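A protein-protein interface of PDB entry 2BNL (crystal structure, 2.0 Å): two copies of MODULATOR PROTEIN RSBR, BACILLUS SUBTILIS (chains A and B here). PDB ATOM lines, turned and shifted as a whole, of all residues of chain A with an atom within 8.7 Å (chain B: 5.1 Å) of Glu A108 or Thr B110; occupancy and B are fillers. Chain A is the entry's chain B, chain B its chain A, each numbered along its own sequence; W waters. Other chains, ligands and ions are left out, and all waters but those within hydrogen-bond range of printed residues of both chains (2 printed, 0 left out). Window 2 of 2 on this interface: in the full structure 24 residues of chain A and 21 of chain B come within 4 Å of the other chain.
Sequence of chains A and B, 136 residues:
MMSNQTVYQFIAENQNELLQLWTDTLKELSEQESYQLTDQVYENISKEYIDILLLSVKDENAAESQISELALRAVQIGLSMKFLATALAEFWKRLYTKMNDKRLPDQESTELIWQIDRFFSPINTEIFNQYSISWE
OH of Tyr A96 touches CG2 of Thr B110, 3.5 Å away. Tyr A96 touches Trp B114. Thr B110 touches Glu A108. Ser A109 touches Thr B110. Ser B109 touches Thr A110. Thr B110 touches Ile A113 (CG2 to CD1, 3.9 Å). CD1 of Ile A113 touches CD1 of Ile B113, 3.8 Å away. Ile A113 touches Trp B114 (CD1 to CZ2, 3.8 Å). CZ2 of Trp A114 touches CD1 of Ile B113, 3.95 Å away.
Glu A108 touches Thr B110, but with the chains exchanged Thr A110 does not touch Glu B108 (5.9 Å). Ser A109 touches Thr B110, and with the chains exchanged Thr A110 touches Ser B109. Ile A113 touches Thr B110, but with the chains exchanged Thr A110 does not touch Ile B113 (4.2 Å). Ile A113 touches its own counterpart, Ile B113. Of the 10 pairs that touch across the chains among the printed residues, 6 have their exchanged pair printed and touching as well.
Of the 11 printed residues of chain A, 6 touch a printed residue of chain B. Hydrophobic or aromatic side chains of chain B that line the printed part of chain A: Ile B113 and Trp B114. Along chain B the printed residues that touch a printed residue of chain A span positions 109 to 114. Among the printed residues, 10 pairs touch across the chains. Among the printed residues, no Asp or Glu carboxylate lies within 4 Å of a Lys or Arg side-chain nitrogen of the other chain.
Water W1 lies within hydrogen-bond range of OH of Tyr A96 (3.0 Å), OE1 of Glu B111 (3.1 Å) and NE1 of Trp B114 (3.2 Å). Water W2 bridges OE2 of Glu A108 (3.1 Å) and OG1 of Thr B110 (3.2 Å).
OG1 of Thr B110 is in hydrogen-bond range of OG1 of Thr A110 (2.9 Å).
Printed residues of chain B within 4 Å of Tyr A96: Thr B110 and Trp B114. Glu A108 touches just one residue of chain B: Thr B110 (3.7 Å). Printed residues of chain B within 4 Å of Ser A109: Thr B110 (3.4 Å). Glu A111 touches none of the printed residues of chain B. Glu B108 touches none of the printed residues of chain A. Of chain A, only Thr A110 (3.1 Å) comes within 4 Å of Ser B109. Thr B110 touches just these residues of chain A: Tyr A96 (3.5 Å), Glu A108 (3.7 Å), Ser A109 (3.4 Å), Thr A110 (2.9 Å) and Ile A113 (3.9 Å). Glu B111 touches none of the printed residues of chain A. Printed residues of chain A within 4 Å of Ile B113: Ile A113 and Trp A114. The nearest printed residue of chain B that does not touch Ser A109 is Ile B113 (6.3 Å).
OH of Tyr A96 is in hydrogen-bond range of OD1 of Asn A100, at 3.3 Å. N of Thr A110 sits at hydrogen-bond distance from OE2 of Glu A108 (3.3 Å). The side-chain amide nitrogen (ND2) of Asn A100 sits at hydrogen-bond distance from the side-chain hydroxyl (OG) of Ser A109, at 2.8 Å.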
ATOM      1  N   TYR A  96       5.920  -0.928 -13.892  1.00  0.00           N
ATOM      2  CA  TYR A  96       6.007   0.222 -14.738  1.00  0.00           C
ATOM      3  C   TYR A  96       6.265   1.525 -13.958  1.00  0.00           C
ATOM      4  O   TYR A  96       7.087   2.328 -14.347  1.00  0.00           O
ATOM      5  CB  TYR A  96       4.749   0.377 -15.639  1.00  0.00           C
ATOM      6  CG  TYR A  96       4.654   1.732 -16.298  1.00  0.00           C
ATOM      7  CD1 TYR A  96       5.378   2.025 -17.405  1.00  0.00           C
ATOM      8  CD2 TYR A  96       3.859   2.711 -15.760  1.00  0.00           C
ATOM      9  CE1 TYR A  96       5.325   3.296 -17.974  1.00  0.00           C
ATOM     10  CE2 TYR A  96       3.748   3.944 -16.350  1.00  0.00           C
ATOM     11  CZ  TYR A  96       4.521   4.226 -17.437  1.00  0.00           C
ATOM     12  OH  TYR A  96       4.396   5.428 -18.011  1.00  0.00           O
ATOM     13  N   MET A  99       9.802   1.595 -12.850  1.00  0.00           N
ATOM     14  CA  MET A  99      10.796   1.818 -13.905  1.00  0.00           C
ATOM     15  C   MET A  99      10.623   3.175 -14.579  1.00  0.00           C
ATOM     16  O   MET A  99      11.601   3.818 -14.953  1.00  0.00           O
ATOM     17  CB  MET A  99      10.797   0.756 -14.969  1.00  0.00           C
ATOM     18  CG  MET A  99      11.080  -0.575 -14.427  1.00  0.00           C
ATOM     19  SD  MET A  99      11.036  -1.845 -15.903  1.00  0.00           S
ATOM     20  CE  MET A  99      12.560  -1.320 -17.077  1.00  0.00           C
ATOM     21  N   ASN A 100       9.383   3.623 -14.730  1.00  0.00           N
ATOM     22  CA  ASN A 100       9.130   4.965 -15.323  1.00  0.00           C
ATOM     23  C   ASN A 100       9.718   6.181 -14.583  1.00  0.00           C
ATOM     24  O   ASN A 100       9.824   7.281 -15.140  1.00  0.00           O
ATOM     25  CB  ASN A 100       7.656   5.187 -15.494  1.00  0.00           C
ATOM     26  CG  ASN A 100       7.342   6.341 -16.465  1.00  0.00           C
ATOM     27  OD1 ASN A 100       6.491   7.130 -16.171  1.00  0.00           O
ATOM     28  ND2 ASN A 100       8.000   6.401 -17.593  1.00  0.00           N
ATOM     29  N   GLU A 108      11.251   7.416 -23.509  1.00  0.00           N
ATOM     30  CA  GLU A 108       9.751   7.443 -23.543  1.00  0.00           C
ATOM     31  C   GLU A 108       9.003   6.350 -22.779  1.00  0.00           C
ATOM     32  O   GLU A 108       9.302   5.152 -22.826  1.00  0.00           O
ATOM     33  CB  GLU A 108       9.196   7.598 -24.963  1.00  0.00           C
ATOM     34  CG  GLU A 108       7.701   7.439 -25.158  1.00  0.00           C
ATOM     35  CD  GLU A 108       6.805   8.698 -24.702  1.00  0.00           C
ATOM     36  OE1 GLU A 108       6.901   9.755 -25.344  1.00  0.00           O
ATOM     37  OE2 GLU A 108       5.964   8.607 -23.750  1.00  0.00           O
ATOM     38  N   SER A 109       7.945   6.828 -22.131  1.00  0.00           N
ATOM     39  CA  SER A 109       7.066   6.067 -21.305  1.00  0.00           C
ATOM     40  C   SER A 109       6.359   4.976 -22.046  1.00  0.00           C
ATOM     41  O   SER A 109       6.325   3.835 -21.606  1.00  0.00           O
ATOM     42  CB  SER A 109       6.058   7.033 -20.735  1.00  0.00           C
ATOM     43  OG  SER A 109       6.719   7.711 -19.686  1.00  0.00           O
ATOM     44  N   THR A 110       5.848   5.351 -23.207  1.00  0.00           N
ATOM     45  CA  THR A 110       5.223   4.433 -24.095  1.00  0.00           C
ATOM     46  C   THR A 110       6.138   3.262 -24.520  1.00  0.00           C
ATOM     47  O   THR A 110       5.718   2.111 -24.515  1.00  0.00           O
ATOM     48  CB  THR A 110       4.617   5.166 -25.348  1.00  0.00           C
ATOM     49  OG1 THR A 110       3.539   6.036 -24.937  1.00  0.00           O
ATOM     50  CG2 THR A 110       4.085   4.136 -26.340  1.00  0.00           C
ATOM     51  N   GLU A 111       7.383   3.537 -24.897  1.00  0.00           N
ATOM     52  CA  GLU A 111       8.270   2.452 -25.264  1.00  0.00           C
ATOM     53  C   GLU A 111       8.551   1.502 -24.115  1.00  0.00           C
ATOM     54  O   GLU A 111       8.686   0.294 -24.313  1.00  0.00           O
ATOM     55  CB  GLU A 111       9.594   2.963 -25.868  1.00  0.00           C
ATOM     56  CG  GLU A 111      10.120   1.996 -27.023  1.00  0.00           C
ATOM     57  CD  GLU A 111       9.160   0.765 -27.394  1.00  0.00           C
ATOM     58  OE1 GLU A 111       8.277   0.974 -28.317  1.00  0.00           O
ATOM     59  OE2 GLU A 111       9.299  -0.397 -26.767  1.00  0.00           O
ATOM     60  N   LEU A 112       8.701   2.049 -22.923  1.00  0.00           N
ATOM     61  CA  LEU A 112       8.824   1.230 -21.686  1.00  0.00           C
ATOM     62  C   LEU A 112       7.643   0.288 -21.490  1.00  0.00           C
ATOM     63  O   LEU A 112       7.848  -0.883 -21.267  1.00  0.00           O
ATOM     64  CB  LEU A 112       9.065   2.170 -20.495  1.00  0.00           C
ATOM     65  CG  LEU A 112       9.066   1.482 -19.127  1.00  0.00           C
ATOM     66  CD1 LEU A 112      10.250   0.520 -19.058  1.00  0.00           C
ATOM     67  CD2 LEU A 112       9.023   2.547 -17.962  1.00  0.00           C
ATOM     68  N   ILE A 113       6.410   0.779 -21.658  1.00  0.00           N
ATOM     69  CA  ILE A 113       5.218  -0.067 -21.600  1.00  0.00           C
ATOM     70  C   ILE A 113       5.275  -1.234 -22.560  1.00  0.00           C
ATOM     71  O   ILE A 113       5.044  -2.404 -22.122  1.00  0.00           O
ATOM     72  CB  ILE A 113       3.895   0.731 -21.828  1.00  0.00           C
ATOM     73  CG1 ILE A 113       3.714   1.700 -20.688  1.00  0.00           C
ATOM     74  CG2 ILE A 113       2.727  -0.208 -21.893  1.00  0.00           C
ATOM     75  CD1 ILE A 113       2.673   2.741 -20.960  1.00  0.00           C
ATOM     76  N   TRP A 114       5.653  -0.947 -23.815  1.00  0.00           N
ATOM     77  CA  TRP A 114       5.821  -1.997 -24.789  1.00  0.00           C
ATOM     78  C   TRP A 114       6.974  -2.979 -24.496  1.00  0.00           C
ATOM     79  O   TRP A 114       6.860  -4.170 -24.806  1.00  0.00           O
ATOM     80  CB  TRP A 114       5.946  -1.414 -26.197  1.00  0.00           C
ATOM     81  CG  TRP A 114       4.731  -0.659 -26.581  1.00  0.00           C
ATOM     82  CD1 TRP A 114       4.669   0.607 -27.096  1.00  0.00           C
ATOM     83  CD2 TRP A 114       3.361  -1.120 -26.495  1.00  0.00           C
ATOM     84  NE1 TRP A 114       3.353   0.961 -27.321  1.00  0.00           N
ATOM     85  CE2 TRP A 114       2.536  -0.074 -26.948  1.00  0.00           C
ATOM     86  CE3 TRP A 114       2.769  -2.311 -26.085  1.00  0.00           C
ATOM     87  CZ2 TRP A 114       1.192  -0.186 -26.997  1.00  0.00           C
ATOM     88  CZ3 TRP A 114       1.408  -2.415 -26.108  1.00  0.00           C
ATOM     89  CH2 TRP A 114       0.627  -1.384 -26.566  1.00  0.00           C
ATOM     90  N   GLN A 115       8.047  -2.510 -23.877  1.00  0.00           N
ATOM     91  CA  GLN A 115       9.104  -3.379 -23.400  1.00  0.00           C
ATOM     92  C   GLN A 115       8.618  -4.296 -22.357  1.00  0.00           C
ATOM     93  O   GLN A 115       8.950  -5.490 -22.335  1.00  0.00           O
ATOM     94  CB  GLN A 115      10.299  -2.592 -22.820  1.00  0.00           C
ATOM     95  CG  GLN A 115      11.187  -1.882 -23.890  1.00  0.00           C
ATOM     96  CD  GLN A 115      12.276  -1.026 -23.207  1.00  0.00           C
ATOM     97  OE1 GLN A 115      12.011  -0.350 -22.226  1.00  0.00           O
ATOM     98  NE2 GLN A 115      13.503  -1.098 -23.727  1.00  0.00           N
ATOM     99  N   GLU B 108      -1.758  12.291 -24.915  1.00  0.00           N
ATOM    100  CA  GLU B 108      -0.574  11.386 -24.720  1.00  0.00           C
ATOM    101  C   GLU B 108      -0.919   9.915 -25.064  1.00  0.00           C
ATOM    102  O   GLU B 108      -1.997   9.388 -24.758  1.00  0.00           O
ATOM    103  CB  GLU B 108       0.056  11.367 -23.289  1.00  0.00           C
ATOM    104  CG  GLU B 108       0.604  12.709 -22.662  1.00  0.00           C
ATOM    105  CD  GLU B 108      -0.235  13.246 -21.433  1.00  0.00           C
ATOM    106  OE1 GLU B 108      -1.228  12.583 -20.957  1.00  0.00           O
ATOM    107  OE2 GLU B 108       0.091  14.361 -20.952  1.00  0.00           O
ATOM    108  N   SER B 109       0.035   9.247 -25.681  1.00  0.00           N
ATOM    109  CA  SER B 109      -0.019   7.804 -25.933  1.00  0.00           C
ATOM    110  C   SER B 109      -0.149   6.964 -24.653  1.00  0.00           C
ATOM    111  O   SER B 109      -0.923   6.024 -24.595  1.00  0.00           O
ATOM    112  CB  SER B 109       1.262   7.382 -26.630  1.00  0.00           C
ATOM    113  OG  SER B 109       1.215   7.926 -27.899  1.00  0.00           O
ATOM    114  N   THR B 110       0.618   7.350 -23.646  1.00  0.00           N
ATOM    115  CA  THR B 110       0.657   6.637 -22.399  1.00  0.00           C
ATOM    116  C   THR B 110      -0.741   6.673 -21.743  1.00  0.00           C
ATOM    117  O   THR B 110      -1.273   5.644 -21.372  1.00  0.00           O
ATOM    118  CB  THR B 110       1.830   7.178 -21.528  1.00  0.00           C
ATOM    119  OG1 THR B 110       3.040   6.864 -22.218  1.00  0.00           O
ATOM    120  CG2 THR B 110       1.911   6.530 -20.173  1.00  0.00           C
ATOM    121  N   GLU B 111      -1.339   7.835 -21.665  1.00  0.00           N
ATOM    122  CA  GLU B 111      -2.683   7.890 -21.116  1.00  0.00           C
ATOM    123  C   GLU B 111      -3.740   7.143 -21.925  1.00  0.00           C
ATOM    124  O   GLU B 111      -4.575   6.511 -21.325  1.00  0.00           O
ATOM    125  CB  GLU B 111      -3.083   9.360 -20.759  1.00  0.00           C
ATOM    126  CG  GLU B 111      -2.040   9.875 -19.592  1.00  0.00           C
ATOM    127  CD  GLU B 111      -1.651   8.780 -18.463  1.00  0.00           C
ATOM    128  OE1 GLU B 111      -0.416   8.477 -18.235  1.00  0.00           O
ATOM    129  OE2 GLU B 111      -2.610   8.233 -17.807  1.00  0.00           O
ATOM    130  N   LEU B 112      -3.660   7.176 -23.256  1.00  0.00           N
ATOM    131  CA  LEU B 112      -4.424   6.274 -24.062  1.00  0.00           C
ATOM    132  C   LEU B 112      -4.281   4.786 -23.724  1.00  0.00           C
ATOM    133  O   LEU B 112      -5.254   4.074 -23.658  1.00  0.00           O
ATOM    134  CB  LEU B 112      -4.115   6.510 -25.542  1.00  0.00           C
ATOM    135  CG  LEU B 112      -4.869   5.613 -26.520  1.00  0.00           C
ATOM    136  CD1 LEU B 112      -6.428   5.780 -26.390  1.00  0.00           C
ATOM    137  CD2 LEU B 112      -4.451   5.924 -27.972  1.00  0.00           C
ATOM    138  N   ILE B 113      -3.065   4.277 -23.570  1.00  0.00           N
ATOM    139  CA  ILE B 113      -2.874   2.942 -23.120  1.00  0.00           C
ATOM    140  C   ILE B 113      -3.564   2.651 -21.785  1.00  0.00           C
ATOM    141  O   ILE B 113      -4.163   1.599 -21.610  1.00  0.00           O
ATOM    142  CB  ILE B 113      -1.358   2.642 -22.981  1.00  0.00           C
ATOM    143  CG1 ILE B 113      -0.703   2.650 -24.369  1.00  0.00           C
ATOM    144  CG2 ILE B 113      -1.108   1.293 -22.200  1.00  0.00           C
ATOM    145  CD1 ILE B 113       0.798   2.657 -24.282  1.00  0.00           C
ATOM    146  N   TRP B 114      -3.411   3.535 -20.820  1.00  0.00           N
ATOM    147  CA  TRP B 114      -4.034   3.296 -19.521  1.00  0.00           C
ATOM    148  C   TRP B 114      -5.581   3.340 -19.572  1.00  0.00           C
ATOM    149  O   TRP B 114      -6.276   2.624 -18.793  1.00  0.00           O
ATOM    150  CB  TRP B 114      -3.422   4.267 -18.500  1.00  0.00           C
ATOM    151  CG  TRP B 114      -1.976   4.028 -18.267  1.00  0.00           C
ATOM    152  CD1 TRP B 114      -1.023   4.957 -18.290  1.00  0.00           C
ATOM    153  CD2 TRP B 114      -1.315   2.786 -17.964  1.00  0.00           C
ATOM    154  NE1 TRP B 114       0.206   4.398 -18.091  1.00  0.00           N
ATOM    155  CE2 TRP B 114       0.056   3.057 -17.896  1.00  0.00           C
ATOM    156  CE3 TRP B 114      -1.750   1.445 -17.792  1.00  0.00           C
ATOM    157  CZ2 TRP B 114       0.988   2.087 -17.607  1.00  0.00           C
ATOM    158  CZ3 TRP B 114      -0.850   0.503 -17.511  1.00  0.00           C
ATOM    159  CH2 TRP B 114       0.530   0.824 -17.417  1.00  0.00           C
HETATM  160  O   HOH W   1       1.965   6.897 -17.047  1.00  0.00           O
HETATM  161  O   HOH W   2       3.030   9.685 -23.825  1.00  0.00           O
